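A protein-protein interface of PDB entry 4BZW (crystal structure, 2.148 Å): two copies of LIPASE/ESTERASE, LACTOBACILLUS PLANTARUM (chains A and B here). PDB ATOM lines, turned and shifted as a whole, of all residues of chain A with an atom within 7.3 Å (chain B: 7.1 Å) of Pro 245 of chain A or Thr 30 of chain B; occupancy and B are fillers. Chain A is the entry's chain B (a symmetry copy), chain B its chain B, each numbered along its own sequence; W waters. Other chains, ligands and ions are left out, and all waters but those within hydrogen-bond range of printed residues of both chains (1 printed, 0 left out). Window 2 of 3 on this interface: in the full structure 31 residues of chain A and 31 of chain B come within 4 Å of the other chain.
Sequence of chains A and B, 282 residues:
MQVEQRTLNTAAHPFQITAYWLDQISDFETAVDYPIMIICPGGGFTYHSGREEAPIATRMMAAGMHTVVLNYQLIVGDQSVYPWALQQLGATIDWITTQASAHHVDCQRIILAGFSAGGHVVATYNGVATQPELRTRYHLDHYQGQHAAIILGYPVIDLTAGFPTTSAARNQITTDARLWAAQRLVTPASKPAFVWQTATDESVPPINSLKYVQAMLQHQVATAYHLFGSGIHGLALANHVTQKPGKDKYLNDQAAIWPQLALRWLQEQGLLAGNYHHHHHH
The side-chain amide nitrogen (NE2) of Gln 243 of chain A lies within hydrogen-bond range of the backbone carbonyl oxygen (O) of Lys 247 of chain A.
Phe 28 of chain B touches Gln 243 of chain A (CZ to O, 3.1 Å). Phe 28 of chain B touches Lys 244 of chain A. CD of Pro 245 of chain A touches CG of Phe 28 of chain B (3.8 Å). CG of Pro 245 of chain A touches OG1 of Thr 30 of chain B, at 3.6 Å.
Printed residues of chain B within 4 Å of Gln 243 of chain A: Phe 28 (3.1 Å). Pro 245 of chain A touches just these residues of chain B: Phe 28 (3.8 Å) and Thr 30 (3.6 Å). Asp 27 of chain B touches none of the printed residues of chain A. Printed residues of chain A within 4 Å of Phe 28 of chain B: Gln 243 (3.1 Å), Lys 244 (3.8 Å) and Pro 245 (3.8 Å). Ala 31 of chain B touches none of the printed residues of chain A. The nearest residue of chain B that does not touch Pro 245 of chain A is Val 32 of chain B (4.1 Å). The nearest residue of chain A that does not touch Thr 30 of chain B is Lys 244 of chain A (6.7 Å).
Printed residues of chain B that touch a printed residue of chain A: Phe 28 and Thr 30. Along chain B the printed residues that touch a printed residue of chain A span positions 28 to 30. Hydrophobic or aromatic side chains of chain A that line the printed part of chain B: Pro 245. Among the printed residues, 4 pairs touch across the chains.
No position is printed for both chains.
Water W1 bridges the backbone carbonyl oxygen of Asp 27 of chain B (2.9 Å) and the side-chain amino group of Lys 244 of chain A (3.0 Å).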
ATOM      1  N   HIS A 240     -11.500  -6.215 -31.397  1.00  0.00           N
ATOM      2  CA  HIS A 240     -12.012  -7.197 -30.438  1.00  0.00           C
ATOM      3  C   HIS A 240     -13.036  -6.619 -29.451  1.00  0.00           C
ATOM      4  O   HIS A 240     -13.904  -7.330 -28.951  1.00  0.00           O
ATOM      5  CB  HIS A 240     -10.854  -7.837 -29.669  1.00  0.00           C
ATOM      6  CG  HIS A 240     -10.165  -6.891 -28.736  1.00  0.00           C
ATOM      7  ND1 HIS A 240     -10.455  -6.830 -27.389  1.00  0.00           N
ATOM      8  CD2 HIS A 240      -9.201  -5.965 -28.955  1.00  0.00           C
ATOM      9  CE1 HIS A 240      -9.693  -5.915 -26.817  1.00  0.00           C
ATOM     10  NE2 HIS A 240      -8.927  -5.371 -27.747  1.00  0.00           N
ATOM     11  N   THR A 242     -15.581  -4.417 -29.936  1.00  0.00           N
ATOM     12  CA  THR A 242     -16.968  -4.404 -30.414  1.00  0.00           C
ATOM     13  C   THR A 242     -17.318  -5.657 -31.208  1.00  0.00           C
ATOM     14  O   THR A 242     -18.378  -5.738 -31.842  1.00  0.00           O
ATOM     15  CB  THR A 242     -17.279  -3.126 -31.235  1.00  0.00           C
ATOM     16  OG1 THR A 242     -16.297  -2.972 -32.270  1.00  0.00           O
ATOM     17  CG2 THR A 242     -17.226  -1.916 -30.333  1.00  0.00           C
ATOM     18  N   GLN A 243     -16.428  -6.641 -31.160  1.00  0.00           N
ATOM     19  CA  GLN A 243     -16.645  -7.884 -31.890  1.00  0.00           C
ATOM     20  C   GLN A 243     -17.677  -8.770 -31.203  1.00  0.00           C
ATOM     21  O   GLN A 243     -17.516  -9.120 -30.028  1.00  0.00           O
ATOM     22  CB  GLN A 243     -15.331  -8.663 -32.025  1.00  0.00           C
ATOM     23  CG  GLN A 243     -15.514 -10.059 -32.609  1.00  0.00           C
ATOM     24  CD  GLN A 243     -14.281 -10.932 -32.462  1.00  0.00           C
ATOM     25  OE1 GLN A 243     -13.385 -10.631 -31.669  1.00  0.00           O
ATOM     26  NE2 GLN A 243     -14.226 -12.019 -33.233  1.00  0.00           N
ATOM     27  N   LYS A 244     -18.728  -9.148 -31.935  1.00  0.00           N
ATOM     28  CA  LYS A 244     -19.671 -10.131 -31.411  1.00  0.00           C
ATOM     29  C   LYS A 244     -18.910 -11.434 -31.185  1.00  0.00           C
ATOM     30  O   LYS A 244     -18.192 -11.898 -32.077  1.00  0.00           O
ATOM     31  CB  LYS A 244     -20.859 -10.333 -32.358  1.00  0.00           C
ATOM     32  CG  LYS A 244     -21.762  -9.109 -32.467  1.00  0.00           C
ATOM     33  CD  LYS A 244     -23.057  -9.410 -33.223  1.00  0.00           C
ATOM     34  CE  LYS A 244     -23.911  -8.151 -33.362  1.00  0.00           C
ATOM     35  NZ  LYS A 244     -25.213  -8.394 -34.055  1.00  0.00           N
ATOM     36  N   PRO A 245     -19.040 -12.007 -29.975  1.00  0.00           N
ATOM     37  CA  PRO A 245     -18.254 -13.164 -29.523  1.00  0.00           C
ATOM     38  C   PRO A 245     -18.208 -14.310 -30.536  1.00  0.00           C
ATOM     39  O   PRO A 245     -19.248 -14.888 -30.859  1.00  0.00           O
ATOM     40  CB  PRO A 245     -18.998 -13.608 -28.259  1.00  0.00           C
ATOM     41  CG  PRO A 245     -19.550 -12.319 -27.701  1.00  0.00           C
ATOM     42  CD  PRO A 245     -19.957 -11.520 -28.925  1.00  0.00           C
ATOM     43  N   GLY A 246     -17.013 -14.620 -31.035  1.00  0.00           N
ATOM     44  CA  GLY A 246     -16.828 -15.738 -31.947  1.00  0.00           C
ATOM     45  C   GLY A 246     -17.052 -15.396 -33.409  1.00  0.00           C
ATOM     46  O   GLY A 246     -16.885 -16.252 -34.282  1.00  0.00           O
ATOM     47  N   LYS A 247     -17.426 -14.150 -33.685  1.00  0.00           N
ATOM     48  CA  LYS A 247     -17.713 -13.726 -35.059  1.00  0.00           C
ATOM     49  C   LYS A 247     -16.560 -12.910 -35.653  1.00  0.00           C
ATOM     50  O   LYS A 247     -16.435 -11.710 -35.385  1.00  0.00           O
ATOM     51  CB  LYS A 247     -19.014 -12.912 -35.122  1.00  0.00           C
ATOM     52  CG  LYS A 247     -20.222 -13.540 -34.423  1.00  0.00           C
ATOM     53  CD  LYS A 247     -20.868 -14.649 -35.237  1.00  0.00           C
ATOM     54  CE  LYS A 247     -22.285 -14.944 -34.734  1.00  0.00           C
ATOM     55  NZ  LYS A 247     -23.171 -13.742 -34.815  1.00  0.00           N
ATOM     56  N   ASP A 248     -15.733 -13.559 -36.468  1.00  0.00           N
ATOM     57  CA  ASP A 248     -14.549 -12.919 -37.040  1.00  0.00           C
ATOM     58  C   ASP A 248     -14.879 -11.775 -37.998  1.00  0.00           C
ATOM     59  O   ASP A 248     -14.064 -10.876 -38.195  1.00  0.00           O
ATOM     60  CB  ASP A 248     -13.653 -13.951 -37.737  1.00  0.00           C
ATOM     61  CG  ASP A 248     -12.796 -14.742 -36.757  1.00  0.00           C
ATOM     62  OD1 ASP A 248     -12.576 -14.255 -35.624  1.00  0.00           O
ATOM     63  OD2 ASP A 248     -12.339 -15.847 -37.121  1.00  0.00           O
ATOM     64  N   TYR A 250     -16.558  -9.266 -37.657  1.00  0.00           N
ATOM     65  CA  TYR A 250     -16.573  -7.954 -37.009  1.00  0.00           C
ATOM     66  C   TYR A 250     -15.173  -7.382 -36.797  1.00  0.00           C
ATOM     67  O   TYR A 250     -15.018  -6.272 -36.278  1.00  0.00           O
ATOM     68  CB  TYR A 250     -17.357  -8.007 -35.695  1.00  0.00           C
ATOM     69  CG  TYR A 250     -18.843  -8.040 -35.941  1.00  0.00           C
ATOM     70  CD1 TYR A 250     -19.524  -6.882 -36.285  1.00  0.00           C
ATOM     71  CD2 TYR A 250     -19.556  -9.232 -35.872  1.00  0.00           C
ATOM     72  CE1 TYR A 250     -20.875  -6.898 -36.532  1.00  0.00           C
ATOM     73  CE2 TYR A 250     -20.912  -9.260 -36.118  1.00  0.00           C
ATOM     74  CZ  TYR A 250     -21.565  -8.086 -36.447  1.00  0.00           C
ATOM     75  OH  TYR A 250     -22.916  -8.090 -36.694  1.00  0.00           O
ATOM     76  N   GLN B  24     -21.535  -4.601 -19.766  1.00  0.00           N
ATOM     77  CA  GLN B  24     -21.741  -5.559 -20.839  1.00  0.00           C
ATOM     78  C   GLN B  24     -22.374  -4.852 -22.036  1.00  0.00           C
ATOM     79  O   GLN B  24     -23.178  -3.933 -21.880  1.00  0.00           O
ATOM     80  CB  GLN B  24     -22.649  -6.694 -20.362  1.00  0.00           C
ATOM     81  CG  GLN B  24     -22.006  -7.595 -19.305  1.00  0.00           C
ATOM     82  CD  GLN B  24     -20.800  -8.325 -19.857  1.00  0.00           C
ATOM     83  OE1 GLN B  24     -20.935  -9.199 -20.709  1.00  0.00           O
ATOM     84  NE2 GLN B  24     -19.611  -7.951 -19.397  1.00  0.00           N
ATOM     85  N   ILE B  25     -22.006  -5.274 -23.235  1.00  0.00           N
ATOM     86  CA  ILE B  25     -22.629  -4.729 -24.428  1.00  0.00           C
ATOM     87  C   ILE B  25     -23.939  -5.485 -24.696  1.00  0.00           C
ATOM     88  O   ILE B  25     -23.923  -6.686 -24.960  1.00  0.00           O
ATOM     89  CB  ILE B  25     -21.671  -4.801 -25.628  1.00  0.00           C
ATOM     90  CG1 ILE B  25     -20.503  -3.823 -25.411  1.00  0.00           C
ATOM     91  CG2 ILE B  25     -22.413  -4.473 -26.917  1.00  0.00           C
ATOM     92  CD1 ILE B  25     -19.265  -4.111 -26.270  1.00  0.00           C
ATOM     93  N   SER B  26     -25.066  -4.782 -24.609  1.00  0.00           N
ATOM     94  CA  SER B  26     -26.384  -5.415 -24.693  1.00  0.00           C
ATOM     95  C   SER B  26     -26.666  -6.144 -26.017  1.00  0.00           C
ATOM     96  O   SER B  26     -27.428  -7.111 -26.034  1.00  0.00           O
ATOM     97  CB  SER B  26     -27.483  -4.390 -24.417  1.00  0.00           C
ATOM     98  OG  SER B  26     -27.413  -3.313 -25.335  1.00  0.00           O
ATOM     99  N   ASP B  27     -26.063  -5.687 -27.119  1.00  0.00           N
ATOM    100  CA  ASP B  27     -26.223  -6.358 -28.419  1.00  0.00           C
ATOM    101  C   ASP B  27     -25.730  -7.798 -28.359  1.00  0.00           C
ATOM    102  O   ASP B  27     -26.240  -8.663 -29.072  1.00  0.00           O
ATOM    103  CB  ASP B  27     -25.406  -5.672 -29.521  1.00  0.00           C
ATOM    104  CG  ASP B  27     -25.812  -4.246 -29.767  1.00  0.00           C
ATOM    105  OD1 ASP B  27     -26.171  -3.549 -28.803  1.00  0.00           O
ATOM    106  OD2 ASP B  27     -25.741  -3.813 -30.936  1.00  0.00           O
ATOM    107  N   PHE B  28     -24.708  -8.041 -27.541  1.00  0.00           N
ATOM    108  CA  PHE B  28     -24.067  -9.353 -27.493  1.00  0.00           C
ATOM    109  C   PHE B  28     -25.055 -10.409 -27.039  1.00  0.00           C
ATOM    110  O   PHE B  28     -25.859 -10.166 -26.138  1.00  0.00           O
ATOM    111  CB  PHE B  28     -22.850  -9.350 -26.555  1.00  0.00           C
ATOM    112  CG  PHE B  28     -21.637  -8.659 -27.127  1.00  0.00           C
ATOM    113  CD1 PHE B  28     -21.685  -8.072 -28.386  1.00  0.00           C
ATOM    114  CD2 PHE B  28     -20.444  -8.610 -26.405  1.00  0.00           C
ATOM    115  CE1 PHE B  28     -20.571  -7.436 -28.921  1.00  0.00           C
ATOM    116  CE2 PHE B  28     -19.321  -7.978 -26.927  1.00  0.00           C
ATOM    117  CZ  PHE B  28     -19.384  -7.388 -28.189  1.00  0.00           C
ATOM    118  N   GLU B  29     -25.003 -11.578 -27.666  1.00  0.00           N
ATOM    119  CA  GLU B  29     -25.897 -12.663 -27.290  1.00  0.00           C
ATOM    120  C   GLU B  29     -25.365 -13.451 -26.089  1.00  0.00           C
ATOM    121  O   GLU B  29     -26.116 -14.175 -25.438  1.00  0.00           O
ATOM    122  CB  GLU B  29     -26.171 -13.577 -28.490  1.00  0.00           C
ATOM    123  CG  GLU B  29     -27.003 -12.901 -29.573  1.00  0.00           C
ATOM    124  CD  GLU B  29     -27.087 -13.708 -30.851  1.00  0.00           C
ATOM    125  OE1 GLU B  29     -26.589 -14.853 -30.875  1.00  0.00           O
ATOM    126  OE2 GLU B  29     -27.652 -13.193 -31.837  1.00  0.00           O
ATOM    127  N   THR B  30     -24.076 -13.295 -25.795  1.00  0.00           N
ATOM    128  CA  THR B  30     -23.469 -13.942 -24.628  1.00  0.00           C
ATOM    129  C   THR B  30     -22.624 -12.943 -23.844  1.00  0.00           C
ATOM    130  O   THR B  30     -22.017 -12.047 -24.423  1.00  0.00           O
ATOM    131  CB  THR B  30     -22.572 -15.142 -25.016  1.00  0.00           C
ATOM    132  OG1 THR B  30     -21.535 -14.699 -25.900  1.00  0.00           O
ATOM    133  CG2 THR B  30     -23.384 -16.250 -25.694  1.00  0.00           C
ATOM    134  N   ALA B  31     -22.586 -13.106 -22.524  1.00  0.00           N
ATOM    135  CA  ALA B  31     -21.771 -12.252 -21.663  1.00  0.00           C
ATOM    136  C   ALA B  31     -20.289 -12.519 -21.909  1.00  0.00           C
ATOM    137  O   ALA B  31     -19.906 -13.617 -22.317  1.00  0.00           O
ATOM    138  CB  ALA B  31     -22.122 -12.485 -20.196  1.00  0.00           C
ATOM    139  N   VAL B  32     -19.455 -11.511 -21.680  1.00  0.00           N
ATOM    140  CA  VAL B  32     -18.012 -11.714 -21.779  1.00  0.00           C
ATOM    141  C   VAL B  32     -17.251 -11.161 -20.570  1.00  0.00           C
ATOM    142  O   VAL B  32     -17.573 -10.081 -20.048  1.00  0.00           O
ATOM    143  CB  VAL B  32     -17.418 -11.225 -23.146  1.00  0.00           C
ATOM    144  CG1 VAL B  32     -18.504 -10.659 -24.075  1.00  0.00           C
ATOM    145  CG2 VAL B  32     -16.283 -10.242 -22.945  1.00  0.00           C
HETATM  146  O   HOH W   1     -26.761  -9.591 -31.816  1.00  0.00           O
